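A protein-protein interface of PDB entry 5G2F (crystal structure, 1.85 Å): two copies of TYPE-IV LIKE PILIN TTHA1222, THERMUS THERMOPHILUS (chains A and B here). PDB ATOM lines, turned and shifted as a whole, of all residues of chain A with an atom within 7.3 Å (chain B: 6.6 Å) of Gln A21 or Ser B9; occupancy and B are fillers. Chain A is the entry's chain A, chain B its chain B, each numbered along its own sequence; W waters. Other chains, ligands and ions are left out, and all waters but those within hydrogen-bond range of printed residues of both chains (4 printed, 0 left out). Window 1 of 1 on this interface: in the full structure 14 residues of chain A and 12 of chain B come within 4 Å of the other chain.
Hydrophobic or aromatic side chains of chain B within 4 Å of the printed part of chain A: Ala B5, Ala B6, Tyr B10, Pro B44 and Leu B83. Of the 21 printed residues of chain A, 11 touch a printed residue of chain B. Printed residues of chain A that touch a printed residue of chain B: Ala A17, Ala A20, Gln A21, Arg A22, Pro A24, Pro A30, Leu A33, Ser A38, Gly A39, Phe A40 and Gly A41. Hydrophobic or aromatic side chains of chain A within 4 Å of the printed part of chain B: Ala A17, Ala A20, Pro A24, Pro A30, Leu A33 and Phe A40.
4 positions are printed for both chains.
O of Ser A38 sits at hydrogen-bond distance from NH1 of Arg B12. The side-chain hydroxyl (OG) of Ser B9 is in hydrogen-bond range of the side-chain amide nitrogen (NE2) of Gln A21, at 3.0 Å. The backbone carbonyl oxygen (O) of Gly A39 is in hydrogen-bond range of the backbone NH (N) of Ser B9 (3.1 Å). The backbone NH (N) of Gly A41 sits at hydrogen-bond distance from the side-chain amide oxygen (OE1) of Gln B8 (2.5 Å). The backbone NH of Phe A40 lies within hydrogen-bond range of the side-chain amide oxygen of Gln B8, 3.3 Å away. The backbone carbonyl oxygen (O) of Ala B6 sits at hydrogen-bond distance from the side-chain amide nitrogen (NE2) of Gln A21. The backbone carbonyl oxygen (O) of Gly A39 sits close to the backbone carbonyl oxygen (O) of Ala B5, at 3.4 Å.
Ala A15 touches none of the printed residues of chain B. Leu A18 touches none of the printed residues of chain B. Printed residues of chain B within 4 Å of Gln A21: Ala B6, Ser B9, Tyr B10, Asn B13, Gln B42 and Pro B44. Printed residues of chain B within 4 Å of Pro A30: Asn B13 (3.2 Å). Of the printed residues of chain B, Gly A39 touches Ala B5 (3.4 Å), Gln B8 (3.1 Å), Ser B9 (3.1 Å), Arg B12 (3.7 Å) and Leu B83 (3.6 Å). Of the printed residues of chain A, Ser B9 touches Ala A17 (3.7 Å), Gln A21 (3.0 Å), Leu A33 (3.998 Å), Gly A39 (3.1 Å) and Phe A40 (3.6 Å). Of the printed residues of chain A, Arg B12 touches Leu A33, Ser A38 and Gly A39. Of the printed residues of chain A, Gln B42 touches Ala A20, Gln A21, Arg A22 and Pro A24. The nearest residue of chain B that does not touch Gln A21 is Ala B5 (5.0 Å). The nearest printed residue of chain A that does not touch Ser B9 is Leu A18 (5.0 Å). The nearest printed residue of chain A that does not touch Pro B44 is Ala A17 (5.6 Å).
The side-chain carboxylate of Glu A19 lies within salt-bridge range of the guanidinium group of Arg A22. NH1 of Arg A22 is in hydrogen-bond range of O of Gly A27, at 2.9 Å. The backbone carbonyl oxygen of Ala B5 lies within hydrogen-bond range of the side-chain hydroxyl of Ser B9 (2.7 Å). The backbone carbonyl oxygen (O) of Ala A17 sits at hydrogen-bond distance from the side-chain amide nitrogen (NE2) of Gln A21 (3.0 Å). The side-chain hydroxyl (OG) of Ser B9 sits at hydrogen-bond distance from the backbone carbonyl oxygen (O) of Ala B6 (3.0 Å).
Ala A17 touches Ser B9 (CB to OG, 3.7 Å). CB of Ala B6 touches CB of Ala A20, 3.97 Å away. Tyr B10 touches Gln A21. O of Gln A21 touches CB of Gln B42 (3.6 Å). Gln B42 touches Pro A24 (OE1 to CD, 3.1 Å). Ser B9 touches Leu A33. Leu A33 touches Arg B12. OD1 of Asn B13 touches CB of Leu A33 (3.4 Å). Phe A40 touches Ser B9 (CE1 to CB, 3.6 Å). N of Gly A41 touches CA of Ala B5, 3.9 Å away.
Water W1 bridges the side-chain amide oxygen of Gln A21 (2.4 Å) and the side-chain amide nitrogen of Asn B13 (3.2 Å). Water W2 bridges O of Ala A20 and NE2 of Gln B42. Water W4 bridges O of Pro A30 (2.7 Å) and ND2 of Asn B13 (3.1 Å). Water W3 bridges the side-chain amide oxygen (OD1) of Asn B13 (2.9 Å) and the backbone NH (N) of Leu A33 (3.1 Å).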
ATOM      1  N   ASN A  13      -6.195   4.831  34.736  1.00  0.00           N
ATOM      2  CA  ASN A  13      -7.233   5.873  34.567  1.00  0.00           C
ATOM      3  C   ASN A  13      -8.029   5.751  33.265  1.00  0.00           C
ATOM      4  O   ASN A  13      -9.252   5.982  33.279  1.00  0.00           O
ATOM      5  CB  ASN A  13      -6.634   7.284  34.758  1.00  0.00           C
ATOM      6  CG  ASN A  13      -6.482   7.642  36.221  1.00  0.00           C
ATOM      7  OD1 ASN A  13      -7.296   7.246  37.056  1.00  0.00           O
ATOM      8  ND2 ASN A  13      -5.453   8.426  36.544  1.00  0.00           N
ATOM      9  N   VAL A  14      -7.376   5.308  32.175  1.00  0.00           N
ATOM     10  CA  VAL A  14      -8.072   5.003  30.926  1.00  0.00           C
ATOM     11  C   VAL A  14      -9.093   3.885  31.158  1.00  0.00           C
ATOM     12  O   VAL A  14     -10.258   3.995  30.798  1.00  0.00           O
ATOM     13  CB  VAL A  14      -7.093   4.626  29.795  1.00  0.00           C
ATOM     14  CG1 VAL A  14      -7.813   4.161  28.545  1.00  0.00           C
ATOM     15  CG2 VAL A  14      -6.208   5.816  29.461  1.00  0.00           C
ATOM     16  N   ALA A  15      -8.636   2.804  31.793  1.00  0.00           N
ATOM     17  CA  ALA A  15      -9.528   1.681  32.125  1.00  0.00           C
ATOM     18  C   ALA A  15     -10.730   2.115  32.975  1.00  0.00           C
ATOM     19  O   ALA A  15     -11.861   1.761  32.651  1.00  0.00           O
ATOM     20  CB  ALA A  15      -8.765   0.600  32.864  1.00  0.00           C
ATOM     21  N   LEU A  16     -10.472   2.850  34.050  1.00  0.00           N
ATOM     22  CA  LEU A  16     -11.573   3.370  34.901  1.00  0.00           C
ATOM     23  C   LEU A  16     -12.568   4.212  34.106  1.00  0.00           C
ATOM     24  O   LEU A  16     -13.775   4.060  34.251  1.00  0.00           O
ATOM     25  CB  LEU A  16     -11.055   4.202  36.059  1.00  0.00           C
ATOM     26  CG  LEU A  16     -10.383   3.411  37.175  1.00  0.00           C
ATOM     27  CD1 LEU A  16      -9.571   4.335  38.072  1.00  0.00           C
ATOM     28  CD2 LEU A  16     -11.413   2.642  37.990  1.00  0.00           C
ATOM     29  N   ALA A  17     -12.054   5.028  33.204  1.00  0.00           N
ATOM     30  CA  ALA A  17     -12.929   5.806  32.327  1.00  0.00           C
ATOM     31  C   ALA A  17     -13.783   4.935  31.393  1.00  0.00           C
ATOM     32  O   ALA A  17     -14.985   5.193  31.184  1.00  0.00           O
ATOM     33  CB  ALA A  17     -12.102   6.802  31.519  1.00  0.00           C
ATOM     34  N   LEU A  18     -13.180   3.899  30.825  1.00  0.00           N
ATOM     35  CA  LEU A  18     -13.904   2.984  29.971  1.00  0.00           C
ATOM     36  C   LEU A  18     -15.007   2.212  30.749  1.00  0.00           C
ATOM     37  O   LEU A  18     -16.116   2.008  30.260  1.00  0.00           O
ATOM     38  CB  LEU A  18     -12.913   1.979  29.311  1.00  0.00           C
ATOM     39  CG  LEU A  18     -12.047   2.525  28.201  1.00  0.00           C
ATOM     40  CD1 LEU A  18     -11.069   1.487  27.705  1.00  0.00           C
ATOM     41  CD2 LEU A  18     -12.864   3.023  26.997  1.00  0.00           C
ATOM     42  N   GLU A  19     -14.682   1.777  31.957  1.00  0.00           N
ATOM     43  CA  GLU A  19     -15.650   1.117  32.819  1.00  0.00           C
ATOM     44  C   GLU A  19     -16.904   1.974  33.017  1.00  0.00           C
ATOM     45  O   GLU A  19     -18.035   1.449  33.021  1.00  0.00           O
ATOM     46  CB  GLU A  19     -15.023   0.736  34.165  1.00  0.00           C
ATOM     47  CG  GLU A  19     -13.937  -0.350  34.108  1.00  0.00           C
ATOM     48  CD  GLU A  19     -14.398  -1.669  33.505  1.00  0.00           C
ATOM     49  OE1 GLU A  19     -15.436  -2.230  33.966  1.00  0.00           O
ATOM     50  OE2 GLU A  19     -13.733  -2.103  32.539  1.00  0.00           O
ATOM     51  N   ALA A  20     -16.697   3.269  33.144  1.00  0.00           N
ATOM     52  CA  ALA A  20     -17.807   4.217  33.355  1.00  0.00           C
ATOM     53  C   ALA A  20     -18.735   4.343  32.171  1.00  0.00           C
ATOM     54  O   ALA A  20     -19.800   4.926  32.295  1.00  0.00           O
ATOM     55  CB  ALA A  20     -17.248   5.575  33.719  1.00  0.00           C
ATOM     56  N   GLN A  21     -18.319   3.862  31.008  1.00  0.00           N
ATOM     57  CA  GLN A  21     -19.159   3.947  29.826  1.00  0.00           C
ATOM     58  C   GLN A  21     -19.933   2.673  29.563  1.00  0.00           C
ATOM     59  O   GLN A  21     -20.653   2.612  28.590  1.00  0.00           O
ATOM     60  CB  GLN A  21     -18.315   4.112  28.573  1.00  0.00           C
ATOM     61  CG  GLN A  21     -17.096   5.003  28.681  1.00  0.00           C
ATOM     62  CD  GLN A  21     -17.440   6.452  28.801  1.00  0.00           C
ATOM     63  OE1 GLN A  21     -18.195   6.959  27.988  1.00  0.00           O
ATOM     64  NE2 GLN A  21     -16.814   7.154  29.766  1.00  0.00           N
ATOM     65  N   ARG A  22     -19.772   1.627  30.375  1.00  0.00           N
ATOM     66  CA  ARG A  22     -20.545   0.380  30.180  1.00  0.00           C
ATOM     67  C   ARG A  22     -22.039   0.554  30.373  1.00  0.00           C
ATOM     68  O   ARG A  22     -22.494   1.209  31.290  1.00  0.00           O
ATOM     69  CB  ARG A  22     -20.116  -0.717  31.133  1.00  0.00           C
ATOM     70  CG  ARG A  22     -18.712  -1.229  30.900  1.00  0.00           C
ATOM     71  CD  ARG A  22     -18.441  -2.348  31.890  1.00  0.00           C
ATOM     72  NE  ARG A  22     -17.061  -2.811  31.795  1.00  0.00           N
ATOM     73  CZ  ARG A  22     -16.573  -3.570  30.824  1.00  0.00           C
ATOM     74  NH1 ARG A  22     -17.370  -4.072  29.874  1.00  0.00           N
ATOM     75  NH2 ARG A  22     -15.301  -3.916  30.826  1.00  0.00           N
ATOM     76  N   ASP A  23     -22.818  -0.076  29.500  1.00  0.00           N
ATOM     77  CA  ASP A  23     -24.234  -0.169  29.740  1.00  0.00           C
ATOM     78  C   ASP A  23     -24.438  -0.922  31.054  1.00  0.00           C
ATOM     79  O   ASP A  23     -23.803  -1.954  31.273  1.00  0.00           O
ATOM     80  CB  ASP A  23     -24.881  -0.898  28.602  1.00  0.00           C
ATOM     81  CG  ASP A  23     -26.358  -1.007  28.779  1.00  0.00           C
ATOM     82  OD1 ASP A  23     -26.850  -1.877  29.551  1.00  0.00           O
ATOM     83  OD2 ASP A  23     -27.064  -0.199  28.164  1.00  0.00           O
ATOM     84  N   PRO A  24     -25.230  -0.385  31.957  1.00  0.00           N
ATOM     85  CA  PRO A  24     -25.317  -1.029  33.282  1.00  0.00           C
ATOM     86  C   PRO A  24     -26.163  -2.341  33.352  1.00  0.00           C
ATOM     87  O   PRO A  24     -26.093  -3.072  34.350  1.00  0.00           O
ATOM     88  CB  PRO A  24     -25.987   0.056  34.143  1.00  0.00           C
ATOM     89  CG  PRO A  24     -26.680   0.937  33.204  1.00  0.00           C
ATOM     90  CD  PRO A  24     -25.880   0.926  31.928  1.00  0.00           C
ATOM     91  N   GLY A  27     -23.451  -4.564  30.134  1.00  0.00           N
ATOM     92  CA  GLY A  27     -22.010  -4.388  30.283  1.00  0.00           C
ATOM     93  C   GLY A  27     -21.292  -3.874  29.040  1.00  0.00           C
ATOM     94  O   GLY A  27     -20.084  -3.629  29.071  1.00  0.00           O
ATOM     95  N   ALA A  28     -22.034  -3.757  27.924  1.00  0.00           N
ATOM     96  CA  ALA A  28     -21.420  -3.492  26.650  1.00  0.00           C
ATOM     97  C   ALA A  28     -20.831  -2.095  26.645  1.00  0.00           C
ATOM     98  O   ALA A  28     -21.400  -1.179  27.225  1.00  0.00           O
ATOM     99  CB  ALA A  28     -22.450  -3.600  25.539  1.00  0.00           C
ATOM    100  N   LEU A  29     -19.703  -1.980  25.982  1.00  0.00           N
ATOM    101  CA  LEU A  29     -18.951  -0.715  25.808  1.00  0.00           C
ATOM    102  C   LEU A  29     -19.093  -0.183  24.421  1.00  0.00           C
ATOM    103  O   LEU A  29     -19.285  -0.966  23.494  1.00  0.00           O
ATOM    104  CB  LEU A  29     -17.445  -1.032  25.876  1.00  0.00           C
ATOM    105  CG  LEU A  29     -16.843  -1.677  27.093  1.00  0.00           C
ATOM    106  CD1 LEU A  29     -15.814  -2.689  26.682  1.00  0.00           C
ATOM    107  CD2 LEU A  29     -16.235  -0.627  27.983  1.00  0.00           C
ATOM    108  N   PRO A  30     -18.968   1.145  24.225  1.00  0.00           N
ATOM    109  CA  PRO A  30     -18.813   1.586  22.823  1.00  0.00           C
ATOM    110  C   PRO A  30     -17.430   1.180  22.344  1.00  0.00           C
ATOM    111  O   PRO A  30     -16.419   1.437  23.000  1.00  0.00           O
ATOM    112  CB  PRO A  30     -18.989   3.099  22.883  1.00  0.00           C
ATOM    113  CG  PRO A  30     -18.852   3.454  24.325  1.00  0.00           C
ATOM    114  CD  PRO A  30     -18.989   2.258  25.180  1.00  0.00           C
ATOM    115  N   LEU A  33     -13.938   3.743  20.273  1.00  0.00           N
ATOM    116  CA  LEU A  33     -12.940   4.648  20.884  1.00  0.00           C
ATOM    117  C   LEU A  33     -11.625   3.853  21.026  1.00  0.00           C
ATOM    118  O   LEU A  33     -11.417   3.143  22.030  1.00  0.00           O
ATOM    119  CB  LEU A  33     -13.472   5.126  22.222  1.00  0.00           C
ATOM    120  CG  LEU A  33     -12.641   6.155  22.999  1.00  0.00           C
ATOM    121  CD1 LEU A  33     -12.297   7.398  22.191  1.00  0.00           C
ATOM    122  CD2 LEU A  33     -13.356   6.562  24.272  1.00  0.00           C
ATOM    123  N   SER A  38      -5.741  10.937  23.699  1.00  0.00           N
ATOM    124  CA  SER A  38      -6.522  12.048  24.215  1.00  0.00           C
ATOM    125  C   SER A  38      -7.837  11.611  24.769  1.00  0.00           C
ATOM    126  O   SER A  38      -8.259  10.489  24.528  1.00  0.00           O
ATOM    127  CB  SER A  38      -6.734  13.112  23.108  1.00  0.00           C
ATOM    128  OG  SER A  38      -7.899  12.755  22.369  1.00  0.00           O
ATOM    129  N   GLY A  39      -8.490  12.514  25.514  1.00  0.00           N
ATOM    130  CA  GLY A  39      -9.818  12.252  26.042  1.00  0.00           C
ATOM    131  C   GLY A  39      -9.845  11.431  27.312  1.00  0.00           C
ATOM    132  O   GLY A  39     -10.917  10.966  27.712  1.00  0.00           O
ATOM    133  N   PHE A  40      -8.679  11.262  27.943  1.00  0.00           N
ATOM    134  CA  PHE A  40      -8.598  10.549  29.198  1.00  0.00           C
ATOM    135  C   PHE A  40      -7.827  11.268  30.276  1.00  0.00           C
ATOM    136  O   PHE A  40      -7.043  10.669  31.041  1.00  0.00           O
ATOM    137  CB  PHE A  40      -8.002   9.145  28.979  1.00  0.00           C
ATOM    138  CG  PHE A  40      -8.845   8.250  28.130  1.00  0.00           C
ATOM    139  CD1 PHE A  40      -9.884   7.504  28.693  1.00  0.00           C
ATOM    140  CD2 PHE A  40      -8.653   8.173  26.775  1.00  0.00           C
ATOM    141  CE1 PHE A  40     -10.669   6.689  27.925  1.00  0.00           C
ATOM    142  CE2 PHE A  40      -9.433   7.345  26.002  1.00  0.00           C
ATOM    143  CZ  PHE A  40     -10.445   6.587  26.584  1.00  0.00           C
ATOM    144  N   GLY A  41      -8.052  12.577  30.367  1.00  0.00           N
ATOM    145  CA  GLY A  41      -7.431  13.360  31.404  1.00  0.00           C
ATOM    146  C   GLY A  41      -6.031  13.695  30.971  1.00  0.00           C
ATOM    147  O   GLY A  41      -5.671  13.553  29.801  1.00  0.00           O
ATOM    148  N   LEU B   4     -12.771  13.457  35.179  1.00  0.00           N
ATOM    149  CA  LEU B   4     -12.432  14.201  33.987  1.00  0.00           C
ATOM    150  C   LEU B   4     -12.258  13.217  32.818  1.00  0.00           C
ATOM    151  O   LEU B   4     -12.761  13.457  31.725  1.00  0.00           O
ATOM    152  CB  LEU B   4     -11.153  15.040  34.175  1.00  0.00           C
ATOM    153  CG  LEU B   4     -10.641  15.743  32.917  1.00  0.00           C
ATOM    154  CD1 LEU B   4     -11.660  16.729  32.318  1.00  0.00           C
ATOM    155  CD2 LEU B   4      -9.293  16.434  33.194  1.00  0.00           C
ATOM    156  N   ALA B   5     -11.518  12.137  33.051  1.00  0.00           N
ATOM    157  CA  ALA B   5     -11.338  11.148  31.984  1.00  0.00           C
ATOM    158  C   ALA B   5     -12.672  10.501  31.574  1.00  0.00           C
ATOM    159  O   ALA B   5     -12.923  10.293  30.406  1.00  0.00           O
ATOM    160  CB  ALA B   5     -10.332  10.094  32.410  1.00  0.00           C
ATOM    161  N   ALA B   6     -13.555  10.235  32.525  1.00  0.00           N
ATOM    162  CA  ALA B   6     -14.832   9.601  32.179  1.00  0.00           C
ATOM    163  C   ALA B   6     -15.674  10.588  31.366  1.00  0.00           C
ATOM    164  O   ALA B   6     -16.268  10.224  30.355  1.00  0.00           O
ATOM    165  CB  ALA B   6     -15.564   9.164  33.431  1.00  0.00           C
ATOM    166  N   GLY B   7     -15.622  11.876  31.731  1.00  0.00           N
ATOM    167  CA  GLY B   7     -16.329  12.883  30.923  1.00  0.00           C
ATOM    168  C   GLY B   7     -15.816  13.108  29.517  1.00  0.00           C
ATOM    169  O   GLY B   7     -16.587  13.200  28.552  1.00  0.00           O
ATOM    170  N   GLN B   8     -14.501  13.301  29.408  1.00  0.00           N
ATOM    171  CA  GLN B   8     -13.892  13.496  28.138  1.00  0.00           C
ATOM    172  C   GLN B   8     -14.170  12.327  27.205  1.00  0.00           C
ATOM    173  O   GLN B   8     -14.465  12.533  26.017  1.00  0.00           O
ATOM    174  CB  GLN B   8     -12.389  13.663  28.292  1.00  0.00           C
ATOM    175  CG  GLN B   8     -11.976  14.992  28.866  1.00  0.00           C
ATOM    176  CD  GLN B   8     -10.477  15.077  29.122  1.00  0.00           C
ATOM    177  OE1 GLN B   8      -9.820  14.076  29.329  1.00  0.00           O
ATOM    178  NE2 GLN B   8      -9.938  16.295  29.140  1.00  0.00           N
ATOM    179  N   SER B   9     -14.012  11.113  27.745  1.00  0.00           N
ATOM    180  CA  SER B   9     -14.200   9.927  26.943  1.00  0.00           C
ATOM    181  C   SER B   9     -15.673   9.814  26.484  1.00  0.00           C
ATOM    182  O   SER B   9     -15.927   9.422  25.366  1.00  0.00           O
ATOM    183  CB  SER B   9     -13.647   8.681  27.676  1.00  0.00           C
ATOM    184  OG  SER B   9     -14.226   8.456  28.939  1.00  0.00           O
ATOM    185  N   TYR B  10     -16.625  10.200  27.332  1.00  0.00           N
ATOM    186  CA  TYR B  10     -18.003  10.219  26.929  1.00  0.00           C
ATOM    187  C   TYR B  10     -18.200  11.175  25.753  1.00  0.00           C
ATOM    188  O   TYR B  10     -18.857  10.835  24.747  1.00  0.00           O
ATOM    189  CB  TYR B  10     -18.928  10.651  28.076  1.00  0.00           C
ATOM    190  CG  TYR B  10     -20.406  10.707  27.689  1.00  0.00           C
ATOM    191  CD1 TYR B  10     -21.142   9.560  27.479  1.00  0.00           C
ATOM    192  CD2 TYR B  10     -21.061  11.931  27.561  1.00  0.00           C
ATOM    193  CE1 TYR B  10     -22.509   9.619  27.151  1.00  0.00           C
ATOM    194  CE2 TYR B  10     -22.393  12.005  27.237  1.00  0.00           C
ATOM    195  CZ  TYR B  10     -23.119  10.852  27.025  1.00  0.00           C
ATOM    196  OH  TYR B  10     -24.454  10.919  26.726  1.00  0.00           O
ATOM    197  N   VAL B  11     -17.634  12.368  25.872  1.00  0.00           N
ATOM    198  CA  VAL B  11     -17.699  13.331  24.750  1.00  0.00           C
ATOM    199  C   VAL B  11     -17.143  12.741  23.451  1.00  0.00           C
ATOM    200  O   VAL B  11     -17.747  12.892  22.395  1.00  0.00           O
ATOM    201  CB  VAL B  11     -17.004  14.668  25.100  1.00  0.00           C
ATOM    202  CG1 VAL B  11     -16.857  15.554  23.880  1.00  0.00           C
ATOM    203  CG2 VAL B  11     -17.780  15.362  26.213  1.00  0.00           C
ATOM    204  N   ARG B  12     -15.979  12.105  23.519  1.00  0.00           N
ATOM    205  CA  ARG B  12     -15.391  11.481  22.317  1.00  0.00           C
ATOM    206  C   ARG B  12     -16.353  10.440  21.743  1.00  0.00           C
ATOM    207  O   ARG B  12     -16.503  10.308  20.519  1.00  0.00           O
ATOM    208  CB  ARG B  12     -14.029  10.899  22.618  1.00  0.00           C
ATOM    209  CG  ARG B  12     -12.926  11.947  22.873  1.00  0.00           C
ATOM    210  CD  ARG B  12     -11.504  11.395  22.918  1.00  0.00           C
ATOM    211  NE  ARG B  12     -11.129  10.760  21.658  1.00  0.00           N
ATOM    212  CZ  ARG B  12     -10.134   9.900  21.490  1.00  0.00           C
ATOM    213  NH1 ARG B  12      -9.368   9.528  22.508  1.00  0.00           N
ATOM    214  NH2 ARG B  12      -9.890   9.413  20.278  1.00  0.00           N
ATOM    215  N   ASN B  13     -17.002   9.673  22.621  1.00  0.00           N
ATOM    216  CA  ASN B  13     -17.995   8.677  22.169  1.00  0.00           C
ATOM    217  C   ASN B  13     -19.253   9.305  21.534  1.00  0.00           C
ATOM    218  O   ASN B  13     -19.793   8.775  20.541  1.00  0.00           O
ATOM    219  CB  ASN B  13     -18.311   7.659  23.316  1.00  0.00           C
ATOM    220  CG  ASN B  13     -17.241   6.542  23.419  1.00  0.00           C
ATOM    221  OD1 ASN B  13     -16.701   6.121  22.412  1.00  0.00           O
ATOM    222  ND2 ASN B  13     -17.007   5.998  24.621  1.00  0.00           N
ATOM    223  N   VAL B  14     -19.714  10.419  22.070  1.00  0.00           N
ATOM    224  CA  VAL B  14     -20.810  11.191  21.422  1.00  0.00           C
ATOM    225  C   VAL B  14     -20.386  11.597  20.006  1.00  0.00           C
ATOM    226  O   VAL B  14     -21.143  11.393  19.029  1.00  0.00           O
ATOM    227  CB  VAL B  14     -21.192  12.448  22.222  1.00  0.00           C
ATOM    228  CG1 VAL B  14     -22.177  13.336  21.489  1.00  0.00           C
ATOM    229  CG2 VAL B  14     -21.801  12.060  23.570  1.00  0.00           C
ATOM    230  N   PHE B  40     -26.952   8.603  23.805  1.00  0.00           N
ATOM    231  CA  PHE B  40     -25.594   8.194  23.452  1.00  0.00           C
ATOM    232  C   PHE B  40     -25.050   7.135  24.401  1.00  0.00           C
ATOM    233  O   PHE B  40     -23.895   7.187  24.779  1.00  0.00           O
ATOM    234  CB  PHE B  40     -24.688   9.424  23.414  1.00  0.00           C
ATOM    235  CG  PHE B  40     -25.090  10.391  22.344  1.00  0.00           C
ATOM    236  CD1 PHE B  40     -24.677  10.206  21.059  1.00  0.00           C
ATOM    237  CD2 PHE B  40     -25.974  11.410  22.620  1.00  0.00           C
ATOM    238  CE1 PHE B  40     -25.067  11.081  20.046  1.00  0.00           C
ATOM    239  CE2 PHE B  40     -26.397  12.260  21.626  1.00  0.00           C
ATOM    240  CZ  PHE B  40     -25.945  12.104  20.331  1.00  0.00           C
ATOM    241  N   GLY B  41     -25.883   6.192  24.798  1.00  0.00           N
ATOM    242  CA  GLY B  41     -25.479   5.114  25.706  1.00  0.00           C
ATOM    243  C   GLY B  41     -25.345   5.592  27.135  1.00  0.00           C
ATOM    244  O   GLY B  41     -25.905   6.609  27.536  1.00  0.00           O
ATOM    245  N   GLN B  42     -24.542   4.878  27.891  1.00  0.00           N
ATOM    246  CA  GLN B  42     -24.332   5.196  29.265  1.00  0.00           C
ATOM    247  C   GLN B  42     -23.539   6.474  29.452  1.00  0.00           C
ATOM    248  O   GLN B  42     -22.418   6.612  28.968  1.00  0.00           O
ATOM    249  CB  GLN B  42     -23.621   4.030  29.946  1.00  0.00           C
ATOM    250  CG  GLN B  42     -23.306   4.275  31.400  1.00  0.00           C
ATOM    251  CD  GLN B  42     -24.519   4.463  32.287  1.00  0.00           C
ATOM    252  OE1 GLN B  42     -25.623   4.035  31.974  1.00  0.00           O
ATOM    253  NE2 GLN B  42     -24.297   5.068  33.442  1.00  0.00           N
ATOM    254  N   ARG B  43     -24.127   7.402  30.205  1.00  0.00           N
ATOM    255  CA  ARG B  43     -23.471   8.654  30.513  1.00  0.00           C
ATOM    256  C   ARG B  43     -22.894   8.658  31.941  1.00  0.00           C
ATOM    257  O   ARG B  43     -23.622   8.469  32.916  1.00  0.00           O
ATOM    258  CB  ARG B  43     -24.479   9.796  30.381  1.00  0.00           C
ATOM    259  CG  ARG B  43     -23.885  11.144  30.766  1.00  0.00           C
ATOM    260  CD  ARG B  43     -24.839  12.310  30.574  1.00  0.00           C
ATOM    261  NE  ARG B  43     -26.184  12.050  31.073  1.00  0.00           N
ATOM    262  CZ  ARG B  43     -26.568  12.154  32.325  1.00  0.00           C
ATOM    263  NH1 ARG B  43     -25.724  12.518  33.249  1.00  0.00           N
ATOM    264  NH2 ARG B  43     -27.798  11.854  32.647  1.00  0.00           N
ATOM    265  N   PRO B  44     -21.584   8.839  32.089  1.00  0.00           N
ATOM    266  CA  PRO B  44     -21.062   8.895  33.458  1.00  0.00           C
ATOM    267  C   PRO B  44     -21.687  10.015  34.273  1.00  0.00           C
ATOM    268  O   PRO B  44     -22.010  11.087  33.706  1.00  0.00           O
ATOM    269  CB  PRO B  44     -19.574   9.146  33.263  1.00  0.00           C
ATOM    270  CG  PRO B  44     -19.273   8.761  31.872  1.00  0.00           C
ATOM    271  CD  PRO B  44     -20.533   8.988  31.070  1.00  0.00           C
ATOM    272  N   LEU B  83     -10.183  18.866  21.369  1.00  0.00           N
ATOM    273  CA  LEU B  83     -10.897  18.641  22.624  1.00  0.00           C
ATOM    274  C   LEU B  83     -10.215  19.568  23.604  1.00  0.00           C
ATOM    275  O   LEU B  83      -9.004  19.512  23.746  1.00  0.00           O
ATOM    276  CB  LEU B  83     -10.784  17.155  23.030  1.00  0.00           C
ATOM    277  CG  LEU B  83     -11.564  16.636  24.240  1.00  0.00           C
ATOM    278  CD1 LEU B  83     -13.055  16.705  24.017  1.00  0.00           C
ATOM    279  CD2 LEU B  83     -11.197  15.207  24.597  1.00  0.00           C
HETATM  280  O   HOH W   1     -19.756   6.385  26.233  1.00  0.00           O
HETATM  281  O   HOH W   2     -21.222   5.462  34.497  1.00  0.00           O
HETATM  282  O   HOH W   3     -17.053   4.099  20.409  1.00  0.00           O
HETATM  283  O   HOH W   4     -15.562   3.244  24.874  1.00  0.00           O
